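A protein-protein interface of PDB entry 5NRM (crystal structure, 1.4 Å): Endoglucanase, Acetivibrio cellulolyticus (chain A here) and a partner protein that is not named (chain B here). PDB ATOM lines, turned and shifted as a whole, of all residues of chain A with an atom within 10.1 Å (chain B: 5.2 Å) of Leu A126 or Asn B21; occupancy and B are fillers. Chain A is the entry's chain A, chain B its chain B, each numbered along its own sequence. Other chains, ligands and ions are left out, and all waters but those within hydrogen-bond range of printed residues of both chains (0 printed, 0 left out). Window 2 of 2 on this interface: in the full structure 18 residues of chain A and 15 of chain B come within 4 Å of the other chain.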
ATOM      1  N   SER A  28     -22.929 -13.901  -9.556  1.00  0.00           N
ATOM      2  CA  SER A  28     -24.045 -14.210 -10.514  1.00  0.00           C
ATOM      3  C   SER A  28     -24.945 -15.335  -9.993  1.00  0.00           C
ATOM      4  O   SER A  28     -24.634 -15.978  -8.971  1.00  0.00           O
ATOM      5  CB  SER A  28     -23.511 -14.651 -11.879  1.00  0.00           C
ATOM      6  OG  SER A  28     -22.878 -15.947 -11.794  1.00  0.00           O
ATOM      7  N   ASN A  30     -24.933 -18.098 -11.186  1.00  0.00           N
ATOM      8  CA  ASN A  30     -24.085 -19.300 -11.237  1.00  0.00           C
ATOM      9  C   ASN A  30     -23.270 -19.514  -9.995  1.00  0.00           C
ATOM     10  O   ASN A  30     -22.657 -20.565  -9.786  1.00  0.00           O
ATOM     11  CB  ASN A  30     -23.185 -19.287 -12.461  1.00  0.00           C
ATOM     12  CG  ASN A  30     -23.984 -19.298 -13.751  1.00  0.00           C
ATOM     13  OD1 ASN A  30     -25.029 -19.894 -13.828  1.00  0.00           O
ATOM     14  ND2 ASN A  30     -23.489 -18.621 -14.755  1.00  0.00           N
ATOM     15  N   GLY A  31     -23.284 -18.524  -9.110  1.00  0.00           N
ATOM     16  CA  GLY A  31     -22.637 -18.693  -7.841  1.00  0.00           C
ATOM     17  C   GLY A  31     -21.098 -18.737  -7.857  1.00  0.00           C
ATOM     18  O   GLY A  31     -20.448 -18.497  -8.893  1.00  0.00           O
ATOM     19  N   ILE A  32     -20.521 -19.049  -6.700  1.00  0.00           N
ATOM     20  CA  ILE A  32     -19.109 -19.288  -6.560  1.00  0.00           C
ATOM     21  C   ILE A  32     -18.917 -20.638  -5.905  1.00  0.00           C
ATOM     22  O   ILE A  32     -19.331 -20.825  -4.740  1.00  0.00           O
ATOM     23  CB  ILE A  32     -18.427 -18.198  -5.719  1.00  0.00           C
ATOM     24  CG1 ILE A  32     -18.509 -16.828  -6.413  1.00  0.00           C
ATOM     25  CG2 ILE A  32     -16.998 -18.585  -5.347  1.00  0.00           C
ATOM     26  CD1 ILE A  32     -17.807 -16.686  -7.731  1.00  0.00           C
ATOM     27  N   SER A  33     -18.292 -21.575  -6.608  1.00  0.00           N
ATOM     28  CA  SER A  33     -17.982 -22.913  -6.114  1.00  0.00           C
ATOM     29  C   SER A  33     -16.548 -23.102  -5.696  1.00  0.00           C
ATOM     30  O   SER A  33     -16.267 -24.065  -4.996  1.00  0.00           O
ATOM     31  CB  SER A  33     -18.327 -23.993  -7.122  1.00  0.00           C
ATOM     32  OG  SER A  33     -19.722 -24.020  -7.406  1.00  0.00           O
ATOM     33  N   THR A  34     -15.642 -22.248  -6.153  1.00  0.00           N
ATOM     34  CA  THR A  34     -14.218 -22.379  -5.771  1.00  0.00           C
ATOM     35  C   THR A  34     -13.599 -21.008  -5.606  1.00  0.00           C
ATOM     36  O   THR A  34     -13.985 -20.054  -6.336  1.00  0.00           O
ATOM     37  CB  THR A  34     -13.364 -23.165  -6.866  1.00  0.00           C
ATOM     38  OG1 THR A  34     -12.772 -22.264  -7.821  1.00  0.00           O
ATOM     39  CG2 THR A  34     -14.147 -24.082  -7.695  1.00  0.00           C
ATOM     40  N   ALA A  35     -12.609 -20.888  -4.747  1.00  0.00           N
ATOM     41  CA  ALA A  35     -11.826 -19.644  -4.640  1.00  0.00           C
ATOM     42  C   ALA A  35     -10.468 -19.935  -4.135  1.00  0.00           C
ATOM     43  O   ALA A  35     -10.329 -20.783  -3.222  1.00  0.00           O
ATOM     44  CB  ALA A  35     -12.512 -18.636  -3.744  1.00  0.00           C
ATOM     45  N   PHE A  78     -11.456 -21.854  -0.773  1.00  0.00           N
ATOM     46  CA  PHE A  78     -12.833 -22.295  -0.630  1.00  0.00           C
ATOM     47  C   PHE A  78     -13.157 -23.307  -1.742  1.00  0.00           C
ATOM     48  O   PHE A  78     -12.770 -23.114  -2.908  1.00  0.00           O
ATOM     49  CB  PHE A  78     -13.845 -21.121  -0.733  1.00  0.00           C
ATOM     50  CG  PHE A  78     -15.270 -21.538  -0.851  1.00  0.00           C
ATOM     51  CD1 PHE A  78     -16.039 -21.981   0.275  1.00  0.00           C
ATOM     52  CD2 PHE A  78     -15.864 -21.592  -2.085  1.00  0.00           C
ATOM     53  CE1 PHE A  78     -17.332 -22.409   0.114  1.00  0.00           C
ATOM     54  CE2 PHE A  78     -17.199 -22.007  -2.260  1.00  0.00           C
ATOM     55  CZ  PHE A  78     -17.930 -22.461  -1.161  1.00  0.00           C
ATOM     56  N   LEU A  79     -13.914 -24.360  -1.405  1.00  0.00           N
ATOM     57  CA  LEU A  79     -14.535 -25.210  -2.395  1.00  0.00           C
ATOM     58  C   LEU A  79     -15.834 -25.745  -1.862  1.00  0.00           C
ATOM     59  O   LEU A  79     -15.889 -26.173  -0.689  1.00  0.00           O
ATOM     60  CB  LEU A  79     -13.557 -26.402  -2.641  1.00  0.00           C
ATOM     61  CG  LEU A  79     -14.063 -27.469  -3.645  1.00  0.00           C
ATOM     62  CD1 LEU A  79     -14.204 -26.918  -5.073  1.00  0.00           C
ATOM     63  CD2 LEU A  79     -13.202 -28.704  -3.627  1.00  0.00           C
ATOM     64  N   ASP A  80     -16.838 -25.797  -2.703  1.00  0.00           N
ATOM     65  CA  ASP A  80     -18.052 -26.562  -2.393  1.00  0.00           C
ATOM     66  C   ASP A  80     -17.756 -28.021  -2.476  1.00  0.00           C
ATOM     67  O   ASP A  80     -17.780 -28.564  -3.563  1.00  0.00           O
ATOM     68  CB  ASP A  80     -19.216 -26.199  -3.339  1.00  0.00           C
ATOM     69  CG  ASP A  80     -20.419 -27.092  -3.173  1.00  0.00           C
ATOM     70  OD1 ASP A  80     -20.453 -27.808  -2.129  1.00  0.00           O
ATOM     71  OD2 ASP A  80     -21.238 -27.134  -4.121  1.00  0.00           O
ATOM     72  N   TYR A  81     -17.417 -28.658  -1.353  1.00  0.00           N
ATOM     73  CA  TYR A  81     -16.978 -30.068  -1.397  1.00  0.00           C
ATOM     74  C   TYR A  81     -18.105 -30.943  -1.951  1.00  0.00           C
ATOM     75  O   TYR A  81     -17.778 -32.028  -2.445  1.00  0.00           O
ATOM     76  CB  TYR A  81     -16.625 -30.584  -0.002  1.00  0.00           C
ATOM     77  CG  TYR A  81     -15.179 -30.367   0.391  1.00  0.00           C
ATOM     78  CD1 TYR A  81     -14.530 -29.151   0.153  1.00  0.00           C
ATOM     79  CD2 TYR A  81     -14.448 -31.361   0.961  1.00  0.00           C
ATOM     80  CE1 TYR A  81     -13.223 -28.950   0.539  1.00  0.00           C
ATOM     81  CE2 TYR A  81     -13.140 -31.149   1.384  1.00  0.00           C
ATOM     82  CZ  TYR A  81     -12.524 -29.956   1.151  1.00  0.00           C
ATOM     83  OH  TYR A  81     -11.224 -29.667   1.520  1.00  0.00           O
ATOM     84  N   THR A  82     -19.371 -30.518  -1.916  1.00  0.00           N
ATOM     85  CA  THR A  82     -20.405 -31.319  -2.524  1.00  0.00           C
ATOM     86  C   THR A  82     -20.364 -31.296  -4.063  1.00  0.00           C
ATOM     87  O   THR A  82     -21.016 -32.127  -4.718  1.00  0.00           O
ATOM     88  CB  THR A  82     -21.842 -30.952  -2.095  1.00  0.00           C
ATOM     89  OG1 THR A  82     -22.279 -29.752  -2.717  1.00  0.00           O
ATOM     90  CG2 THR A  82     -21.951 -30.853  -0.558  1.00  0.00           C
ATOM     91  N   MET A  83     -19.773 -30.255  -4.607  1.00  0.00           N
ATOM     92  CA  MET A  83     -19.751 -29.988  -6.068  1.00  0.00           C
ATOM     93  C   MET A  83     -21.171 -30.077  -6.625  1.00  0.00           C
ATOM     94  O   MET A  83     -21.393 -30.643  -7.718  1.00  0.00           O
ATOM     95  CB  MET A  83     -18.771 -30.921  -6.790  1.00  0.00           C
ATOM     96  CG  MET A  83     -17.312 -30.760  -6.353  1.00  0.00           C
ATOM     97  SD  MET A  83     -16.655 -29.226  -7.030  1.00  0.00           S
ATOM     98  CE  MET A  83     -16.784 -29.408  -8.751  1.00  0.00           C
ATOM     99  N   SER A  84     -22.142 -29.503  -5.929  1.00  0.00           N
ATOM    100  CA  SER A  84     -23.519 -29.642  -6.335  1.00  0.00           C
ATOM    101  C   SER A  84     -24.378 -28.471  -5.955  1.00  0.00           C
ATOM    102  O   SER A  84     -24.601 -27.576  -6.744  1.00  0.00           O
ATOM    103  CB  SER A  84     -24.085 -30.962  -5.799  1.00  0.00           C
ATOM    104  OG  SER A  84     -25.460 -30.999  -6.093  1.00  0.00           O
ATOM    105  N   THR A  85     -24.783 -28.361  -4.718  1.00  0.00           N
ATOM    106  CA  THR A  85     -25.671 -27.226  -4.384  1.00  0.00           C
ATOM    107  C   THR A  85     -25.128 -26.417  -3.239  1.00  0.00           C
ATOM    108  O   THR A  85     -25.826 -25.671  -2.588  1.00  0.00           O
ATOM    109  CB  THR A  85     -27.010 -27.759  -3.944  1.00  0.00           C
ATOM    110  OG1 THR A  85     -26.733 -28.731  -2.906  1.00  0.00           O
ATOM    111  CG2 THR A  85     -27.744 -28.387  -5.185  1.00  0.00           C
ATOM    112  N   TYR A  87     -22.650 -24.088  -3.556  1.00  0.00           N
ATOM    113  CA  TYR A  87     -22.008 -22.865  -3.988  1.00  0.00           C
ATOM    114  C   TYR A  87     -22.524 -21.659  -3.180  1.00  0.00           C
ATOM    115  O   TYR A  87     -23.629 -21.662  -2.638  1.00  0.00           O
ATOM    116  CB  TYR A  87     -22.142 -22.589  -5.487  1.00  0.00           C
ATOM    117  CG  TYR A  87     -23.498 -22.744  -6.057  1.00  0.00           C
ATOM    118  CD1 TYR A  87     -23.954 -24.000  -6.439  1.00  0.00           C
ATOM    119  CD2 TYR A  87     -24.356 -21.674  -6.148  1.00  0.00           C
ATOM    120  CE1 TYR A  87     -25.238 -24.165  -6.958  1.00  0.00           C
ATOM    121  CE2 TYR A  87     -25.613 -21.816  -6.655  1.00  0.00           C
ATOM    122  CZ  TYR A  87     -26.058 -23.038  -7.046  1.00  0.00           C
ATOM    123  OH  TYR A  87     -27.348 -23.085  -7.528  1.00  0.00           O
ATOM    124  N   THR A 120      -8.205 -16.659  -8.121  1.00  0.00           N
ATOM    125  CA  THR A 120      -9.070 -17.474  -8.924  1.00  0.00           C
ATOM    126  C   THR A 120     -10.410 -17.778  -8.256  1.00  0.00           C
ATOM    127  O   THR A 120     -10.450 -18.110  -7.083  1.00  0.00           O
ATOM    128  CB  THR A 120      -8.398 -18.788  -9.324  1.00  0.00           C
ATOM    129  OG1 THR A 120      -7.202 -18.485 -10.065  1.00  0.00           O
ATOM    130  CG2 THR A 120      -9.340 -19.711 -10.163  1.00  0.00           C
ATOM    131  N   PHE A 121     -11.481 -17.553  -9.021  1.00  0.00           N
ATOM    132  CA  PHE A 121     -12.851 -17.941  -8.643  1.00  0.00           C
ATOM    133  C   PHE A 121     -13.466 -18.742  -9.724  1.00  0.00           C
ATOM    134  O   PHE A 121     -13.286 -18.436 -10.940  1.00  0.00           O
ATOM    135  CB  PHE A 121     -13.695 -16.687  -8.420  1.00  0.00           C
ATOM    136  CG  PHE A 121     -13.217 -15.872  -7.281  1.00  0.00           C
ATOM    137  CD1 PHE A 121     -13.668 -16.091  -5.988  1.00  0.00           C
ATOM    138  CD2 PHE A 121     -12.298 -14.864  -7.509  1.00  0.00           C
ATOM    139  CE1 PHE A 121     -13.180 -15.334  -4.945  1.00  0.00           C
ATOM    140  CE2 PHE A 121     -11.814 -14.090  -6.459  1.00  0.00           C
ATOM    141  CZ  PHE A 121     -12.262 -14.328  -5.185  1.00  0.00           C
ATOM    142  N   GLY A 122     -14.073 -19.841  -9.326  1.00  0.00           N
ATOM    143  CA  GLY A 122     -14.838 -20.628 -10.261  1.00  0.00           C
ATOM    144  C   GLY A 122     -16.275 -20.645  -9.928  1.00  0.00           C
ATOM    145  O   GLY A 122     -16.614 -20.780  -8.732  1.00  0.00           O
ATOM    146  N   ASP A 123     -17.126 -20.495 -10.941  1.00  0.00           N
ATOM    147  CA  ASP A 123     -18.564 -20.624 -10.713  1.00  0.00           C
ATOM    148  C   ASP A 123     -19.025 -22.071 -10.553  1.00  0.00           C
ATOM    149  O   ASP A 123     -18.192 -22.975 -10.498  1.00  0.00           O
ATOM    150  CB  ASP A 123     -19.336 -19.774 -11.691  1.00  0.00           C
ATOM    151  CG  ASP A 123     -19.418 -20.386 -13.078  1.00  0.00           C
ATOM    152  OD1 ASP A 123     -19.016 -21.552 -13.328  1.00  0.00           O
ATOM    153  OD2 ASP A 123     -19.916 -19.645 -13.968  1.00  0.00           O
ATOM    154  N   SER A 124     -20.353 -22.308 -10.508  1.00  0.00           N
ATOM    155  CA  SER A 124     -20.846 -23.666 -10.210  1.00  0.00           C
ATOM    156  C   SER A 124     -20.615 -24.625 -11.427  1.00  0.00           C
ATOM    157  O   SER A 124     -20.787 -25.842 -11.251  1.00  0.00           O
ATOM    158  CB  SER A 124     -22.318 -23.651  -9.791  1.00  0.00           C
ATOM    159  OG  SER A 124     -23.145 -23.102 -10.799  1.00  0.00           O
ATOM    160  N   THR A 125     -20.299 -24.031 -12.612  1.00  0.00           N
ATOM    161  CA  THR A 125     -19.853 -24.736 -13.829  1.00  0.00           C
ATOM    162  C   THR A 125     -18.333 -24.929 -13.893  1.00  0.00           C
ATOM    163  O   THR A 125     -17.818 -25.451 -14.932  1.00  0.00           O
ATOM    164  CB  THR A 125     -20.399 -24.038 -15.146  1.00  0.00           C
ATOM    165  OG1 THR A 125     -19.711 -22.844 -15.482  1.00  0.00           O
ATOM    166  CG2 THR A 125     -21.907 -23.728 -15.046  1.00  0.00           C
ATOM    167  N   LEU A 126     -17.616 -24.439 -12.897  1.00  0.00           N
ATOM    168  CA  LEU A 126     -16.172 -24.389 -12.836  1.00  0.00           C
ATOM    169  C   LEU A 126     -15.573 -23.527 -13.912  1.00  0.00           C
ATOM    170  O   LEU A 126     -14.424 -23.751 -14.379  1.00  0.00           O
ATOM    171  CB  LEU A 126     -15.571 -25.780 -12.811  1.00  0.00           C
ATOM    172  CG  LEU A 126     -16.042 -26.634 -11.639  1.00  0.00           C
ATOM    173  CD1 LEU A 126     -15.320 -27.994 -11.664  1.00  0.00           C
ATOM    174  CD2 LEU A 126     -15.876 -25.926 -10.303  1.00  0.00           C
ATOM    175  N   THR A 127     -16.341 -22.562 -14.354  1.00  0.00           N
ATOM    176  CA  THR A 127     -15.825 -21.544 -15.259  1.00  0.00           C
ATOM    177  C   THR A 127     -15.207 -20.417 -14.454  1.00  0.00           C
ATOM    178  O   THR A 127     -15.763 -19.975 -13.447  1.00  0.00           O
ATOM    179  CB  THR A 127     -16.940 -20.953 -16.110  1.00  0.00           C
ATOM    180  OG1 THR A 127     -17.451 -22.045 -16.873  1.00  0.00           O
ATOM    181  CG2 THR A 127     -16.428 -19.907 -17.135  1.00  0.00           C
ATOM    182  N   PRO A 128     -14.008 -19.939 -14.844  1.00  0.00           N
ATOM    183  CA  PRO A 128     -13.422 -18.829 -14.140  1.00  0.00           C
ATOM    184  C   PRO A 128     -14.255 -17.550 -14.245  1.00  0.00           C
ATOM    185  O   PRO A 128     -14.805 -17.279 -15.306  1.00  0.00           O
ATOM    186  CB  PRO A 128     -12.072 -18.641 -14.829  1.00  0.00           C
ATOM    187  CG  PRO A 128     -11.859 -19.844 -15.579  1.00  0.00           C
ATOM    188  CD  PRO A 128     -13.210 -20.332 -16.005  1.00  0.00           C
ATOM    189  N   VAL A 129     -14.329 -16.870 -13.110  1.00  0.00           N
ATOM    190  CA  VAL A 129     -15.018 -15.592 -12.966  1.00  0.00           C
ATOM    191  C   VAL A 129     -13.959 -14.568 -12.602  1.00  0.00           C
ATOM    192  O   VAL A 129     -13.351 -14.722 -11.530  1.00  0.00           O
ATOM    193  CB  VAL A 129     -16.035 -15.570 -11.811  1.00  0.00           C
ATOM    194  CG1 VAL A 129     -16.891 -14.292 -11.944  1.00  0.00           C
ATOM    195  CG2 VAL A 129     -16.871 -16.814 -11.799  1.00  0.00           C
ATOM    196  N   ILE B  14      -9.629 -24.179  -9.142  1.00  0.00           N
ATOM    197  CA  ILE B  14     -10.362 -24.918 -10.207  1.00  0.00           C
ATOM    198  C   ILE B  14      -9.736 -26.321 -10.447  1.00  0.00           C
ATOM    199  O   ILE B  14     -10.473 -27.285 -10.600  1.00  0.00           O
ATOM    200  CB  ILE B  14     -10.506 -24.080 -11.488  1.00  0.00           C
ATOM    201  CG1 ILE B  14     -11.467 -22.874 -11.175  1.00  0.00           C
ATOM    202  CG2 ILE B  14     -10.940 -24.958 -12.629  1.00  0.00           C
ATOM    203  CD1 ILE B  14     -11.623 -21.845 -12.297  1.00  0.00           C
ATOM    204  N   ALA B  17     -11.095 -28.280  -7.515  1.00  0.00           N
ATOM    205  CA  ALA B  17     -12.445 -28.681  -7.842  1.00  0.00           C
ATOM    206  C   ALA B  17     -12.569 -29.861  -8.818  1.00  0.00           C
ATOM    207  O   ALA B  17     -13.391 -30.797  -8.642  1.00  0.00           O
ATOM    208  CB  ALA B  17     -13.229 -27.498  -8.344  1.00  0.00           C
ATOM    209  N   LEU B  18     -11.753 -29.837  -9.843  1.00  0.00           N
ATOM    210  CA  LEU B  18     -11.748 -30.911 -10.782  1.00  0.00           C
ATOM    211  C   LEU B  18     -11.287 -32.197 -10.106  1.00  0.00           C
ATOM    212  O   LEU B  18     -11.839 -33.259 -10.358  1.00  0.00           O
ATOM    213  CB  LEU B  18     -10.849 -30.618 -11.975  1.00  0.00           C
ATOM    214  CG  LEU B  18     -11.410 -29.511 -12.902  1.00  0.00           C
ATOM    215  CD1 LEU B  18     -10.371 -29.012 -13.840  1.00  0.00           C
ATOM    216  CD2 LEU B  18     -12.597 -29.956 -13.742  1.00  0.00           C
ATOM    217  N   MET B  19     -10.281 -32.104  -9.274  1.00  0.00           N
ATOM    218  CA  MET B  19      -9.872 -33.274  -8.502  1.00  0.00           C
ATOM    219  C   MET B  19     -11.042 -33.790  -7.615  1.00  0.00           C
ATOM    220  O   MET B  19     -11.240 -34.979  -7.440  1.00  0.00           O
ATOM    221  CB  MET B  19      -8.731 -32.931  -7.629  1.00  0.00           C
ATOM    222  CG  MET B  19      -7.490 -32.647  -8.402  1.00  0.00           C
ATOM    223  SD  MET B  19      -6.110 -32.363  -7.283  1.00  0.00           S
ATOM    224  CE  MET B  19      -5.944 -34.069  -6.651  1.00  0.00           C
ATOM    225  N   ARG B  20     -11.827 -32.842  -7.047  1.00  0.00           N
ATOM    226  CA  ARG B  20     -12.983 -33.262  -6.207  1.00  0.00           C
ATOM    227  C   ARG B  20     -14.000 -33.984  -7.068  1.00  0.00           C
ATOM    228  O   ARG B  20     -14.484 -35.066  -6.702  1.00  0.00           O
ATOM    229  CB  ARG B  20     -13.642 -32.036  -5.544  1.00  0.00           C
ATOM    230  CG  ARG B  20     -14.752 -32.370  -4.561  1.00  0.00           C
ATOM    231  CD  ARG B  20     -14.225 -33.037  -3.284  1.00  0.00           C
ATOM    232  NE  ARG B  20     -15.330 -33.336  -2.373  1.00  0.00           N
ATOM    233  CZ  ARG B  20     -15.252 -34.154  -1.331  1.00  0.00           C
ATOM    234  NH1 ARG B  20     -14.083 -34.636  -0.965  1.00  0.00           N
ATOM    235  NH2 ARG B  20     -16.329 -34.417  -0.607  1.00  0.00           N
ATOM    236  N   ASN B  21     -14.271 -33.448  -8.254  1.00  0.00           N
ATOM    237  CA  ASN B  21     -15.214 -34.127  -9.122  1.00  0.00           C
ATOM    238  C   ASN B  21     -14.737 -35.485  -9.537  1.00  0.00           C
ATOM    239  O   ASN B  21     -15.562 -36.405  -9.665  1.00  0.00           O
ATOM    240  CB  ASN B  21     -15.525 -33.330 -10.351  1.00  0.00           C
ATOM    241  CG  ASN B  21     -16.623 -32.353 -10.133  1.00  0.00           C
ATOM    242  OD1 ASN B  21     -16.705 -31.333 -10.834  1.00  0.00           O
ATOM    243  ND2 ASN B  21     -17.491 -32.645  -9.192  1.00  0.00           N
ATOM    244  N   TYR B  22     -13.418 -35.647  -9.722  1.00  0.00           N
ATOM    245  CA  TYR B  22     -12.850 -36.955 -10.091  1.00  0.00           C
ATOM    246  C   TYR B  22     -13.069 -37.952  -8.938  1.00  0.00           C
ATOM    247  O   TYR B  22     -13.558 -39.099  -9.131  1.00  0.00           O
ATOM    248  CB  TYR B  22     -11.357 -36.803 -10.392  1.00  0.00           C
ATOM    249  CG  TYR B  22     -10.655 -38.060 -10.881  1.00  0.00           C
ATOM    250  CD1 TYR B  22     -10.203 -39.016  -9.981  1.00  0.00           C
ATOM    251  CD2 TYR B  22     -10.361 -38.230 -12.241  1.00  0.00           C
ATOM    252  CE1 TYR B  22      -9.536 -40.155 -10.420  1.00  0.00           C
ATOM    253  CE2 TYR B  22      -9.688 -39.362 -12.689  1.00  0.00           C
ATOM    254  CZ  TYR B  22      -9.289 -40.301 -11.764  1.00  0.00           C
ATOM    255  OH  TYR B  22      -8.603 -41.421 -12.149  1.00  0.00           O
ATOM    256  N   LEU B  23     -12.706 -37.536  -7.721  1.00  0.00           N
ATOM    257  CA  LEU B  23     -12.956 -38.368  -6.507  1.00  0.00           C
ATOM    258  C   LEU B  23     -14.355 -38.751  -6.250  1.00  0.00           C
ATOM    259  O   LEU B  23     -14.608 -39.830  -5.636  1.00  0.00           O
ATOM    260  CB  LEU B  23     -12.535 -37.660  -5.223  1.00  0.00           C
ATOM    261  CG  LEU B  23     -11.065 -37.492  -5.263  1.00  0.00           C
ATOM    262  CD1 LEU B  23     -10.702 -36.794  -3.959  1.00  0.00           C
ATOM    263  CD2 LEU B  23     -10.417 -38.846  -5.493  1.00  0.00           C
ATOM    264  N   LEU B  24     -15.257 -37.830  -6.564  1.00  0.00           N
ATOM    265  CA  LEU B  24     -16.649 -38.047  -6.362  1.00  0.00           C
ATOM    266  C   LEU B  24     -17.220 -38.981  -7.429  1.00  0.00           C
ATOM    267  O   LEU B  24     -18.379 -39.364  -7.366  1.00  0.00           O
ATOM    268  CB  LEU B  24     -17.421 -36.736  -6.318  1.00  0.00           C
ATOM    269  CG  LEU B  24     -17.137 -35.756  -5.157  1.00  0.00           C
ATOM    270  CD1 LEU B  24     -18.043 -34.551  -5.404  1.00  0.00           C
ATOM    271  CD2 LEU B  24     -17.292 -36.317  -3.773  1.00  0.00           C
ATOM    272  N   GLY B  25     -16.411 -39.256  -8.450  1.00  0.00           N
ATOM    273  CA  GLY B  25     -16.806 -40.143  -9.510  1.00  0.00           C
ATOM    274  C   GLY B  25     -17.627 -39.422 -10.537  1.00  0.00           C
ATOM    275  O   GLY B  25     -18.211 -40.112 -11.364  1.00  0.00           O
ATOM    276  N   ASN B  26     -17.625 -38.085 -10.542  1.00  0.00           N
ATOM    277  CA  ASN B  26     -18.385 -37.243 -11.492  1.00  0.00           C
ATOM    278  C   ASN B  26     -17.603 -36.868 -12.772  1.00  0.00           C
ATOM    279  O   ASN B  26     -18.188 -36.448 -13.783  1.00  0.00           O
ATOM    280  CB  ASN B  26     -18.754 -35.902 -10.866  1.00  0.00           C
ATOM    281  CG  ASN B  26     -19.551 -36.037  -9.612  1.00  0.00           C
ATOM    282  OD1 ASN B  26     -20.182 -37.062  -9.373  1.00  0.00           O
ATOM    283  ND2 ASN B  26     -19.503 -34.980  -8.762  1.00  0.00           N
ATOM    284  N   LEU B  27     -16.290 -36.961 -12.696  1.00  0.00           N
ATOM    285  CA  LEU B  27     -15.404 -36.664 -13.827  1.00  0.00           C
ATOM    286  C   LEU B  27     -14.502 -37.852 -13.991  1.00  0.00           C
ATOM    287  O   LEU B  27     -13.914 -38.302 -13.035  1.00  0.00           O
ATOM    288  CB  LEU B  27     -14.578 -35.404 -13.517  1.00  0.00           C
ATOM    289  CG  LEU B  27     -13.485 -34.970 -14.502  1.00  0.00           C
ATOM    290  CD1 LEU B  27     -14.079 -34.704 -15.879  1.00  0.00           C
ATOM    291  CD2 LEU B  27     -12.806 -33.712 -13.974  1.00  0.00           C
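Among the printed residues, pairs that only touch across the chains: Met A83 with Asn B21 (2.8 Å), Leu A79 with Ala B17 (3.5 Å), Met A83 with Arg B20 (3.5 Å), Thr A34 with Ala B17 (3.6 Å), Leu A126 with Ala B17 (3.6 Å), Thr A34 with Ile B14 (3.7 Å), Met A83 with Ala B17 (3.7 Å), Leu A126 with Asn B21 (3.7 Å), Thr A120 with Ile B14 (3.8 Å), Pro A128 with Ile B14 (3.9 Å), Leu A79 with Arg B20 (3.9 Å), Thr A82 with Leu B24 (3.9 Å), Tyr A81 with Leu B24 (3.9 Å), Leu A126 with Leu B18 (3.9 Å), Met A83 with Leu B24 (3.95 Å), Leu A126 with Ile B14 (3.98 Å) and Gly A122 with Ile B14 (3.995 Å).
Hydrophobic or aromatic side chains of chain B within 4 Å of the printed part of chain A: Ile B14, Ala B17, Leu B18 and Leu B24.
Hydrophobic or aromatic side chains of chain A within 4 Å of the printed part of chain B: Leu A79, Tyr A81, Met A83, Leu A126 and Pro A128.
Among the printed residues, 18 pairs touch across the chains.
Among the printed residues, no Asp or Glu carboxylate lies within 4 Å of a Lys or Arg side-chain nitrogen of the other chain.
Of chain A, only Met A83 and Leu A126 come within 4 Å of Asn B21.
Of chain A, only Thr A34, Leu A79, Met A83 and Leu A126 come within 4 Å of Ala B17.
Leu B18 touches just one residue of chain A: Leu A126 (3.9 Å).
Gly B25 touches none of the printed residues of chain A.
No residue of chain A comes within 4 Å of Leu B27.
Of the printed residues of chain B, Thr A120 touches Ile B14.
Of the printed residues of chain A, Ile B14 touches Thr A34, Thr A120, Gly A122, Leu A126 and Pro A128.
Printed residues of chain B within 4 Å of Pro A128: Ile B14.
The nearest printed residue of chain B that does not touch Leu A126 is Leu B27 (6.7 Å).
The nearest residue of chain A that does not touch Asn B21 is Thr A82 (5.7 Å).
The nearest printed residue of chain B that does not touch Leu A79 is Leu B18 (6.1 Å).
O of Tyr A81 lies within hydrogen-bond range of NE of Arg B20, 2.8 Å away.
The backbone NH (N) of Ser A33 sits at hydrogen-bond distance from the backbone carbonyl oxygen (O) of Gly A122 (2.8 Å).
OD2 of Asp A80 sits at hydrogen-bond distance from N of Met A83.
OG1 of Thr A82 lies close to N of Ser A84 (3.2 Å).
The backbone NH (N) of Thr A85 lies within hydrogen-bond range of the side-chain hydroxyl (OG1) of Thr A82.
The backbone carbonyl oxygen of Asn B21 sits at hydrogen-bond distance from the backbone NH of Asn B26.
The backbone carbonyl oxygen (O) of Asn B21 sits at hydrogen-bond distance from the backbone NH (N) of Leu B27 (3.2 Å).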
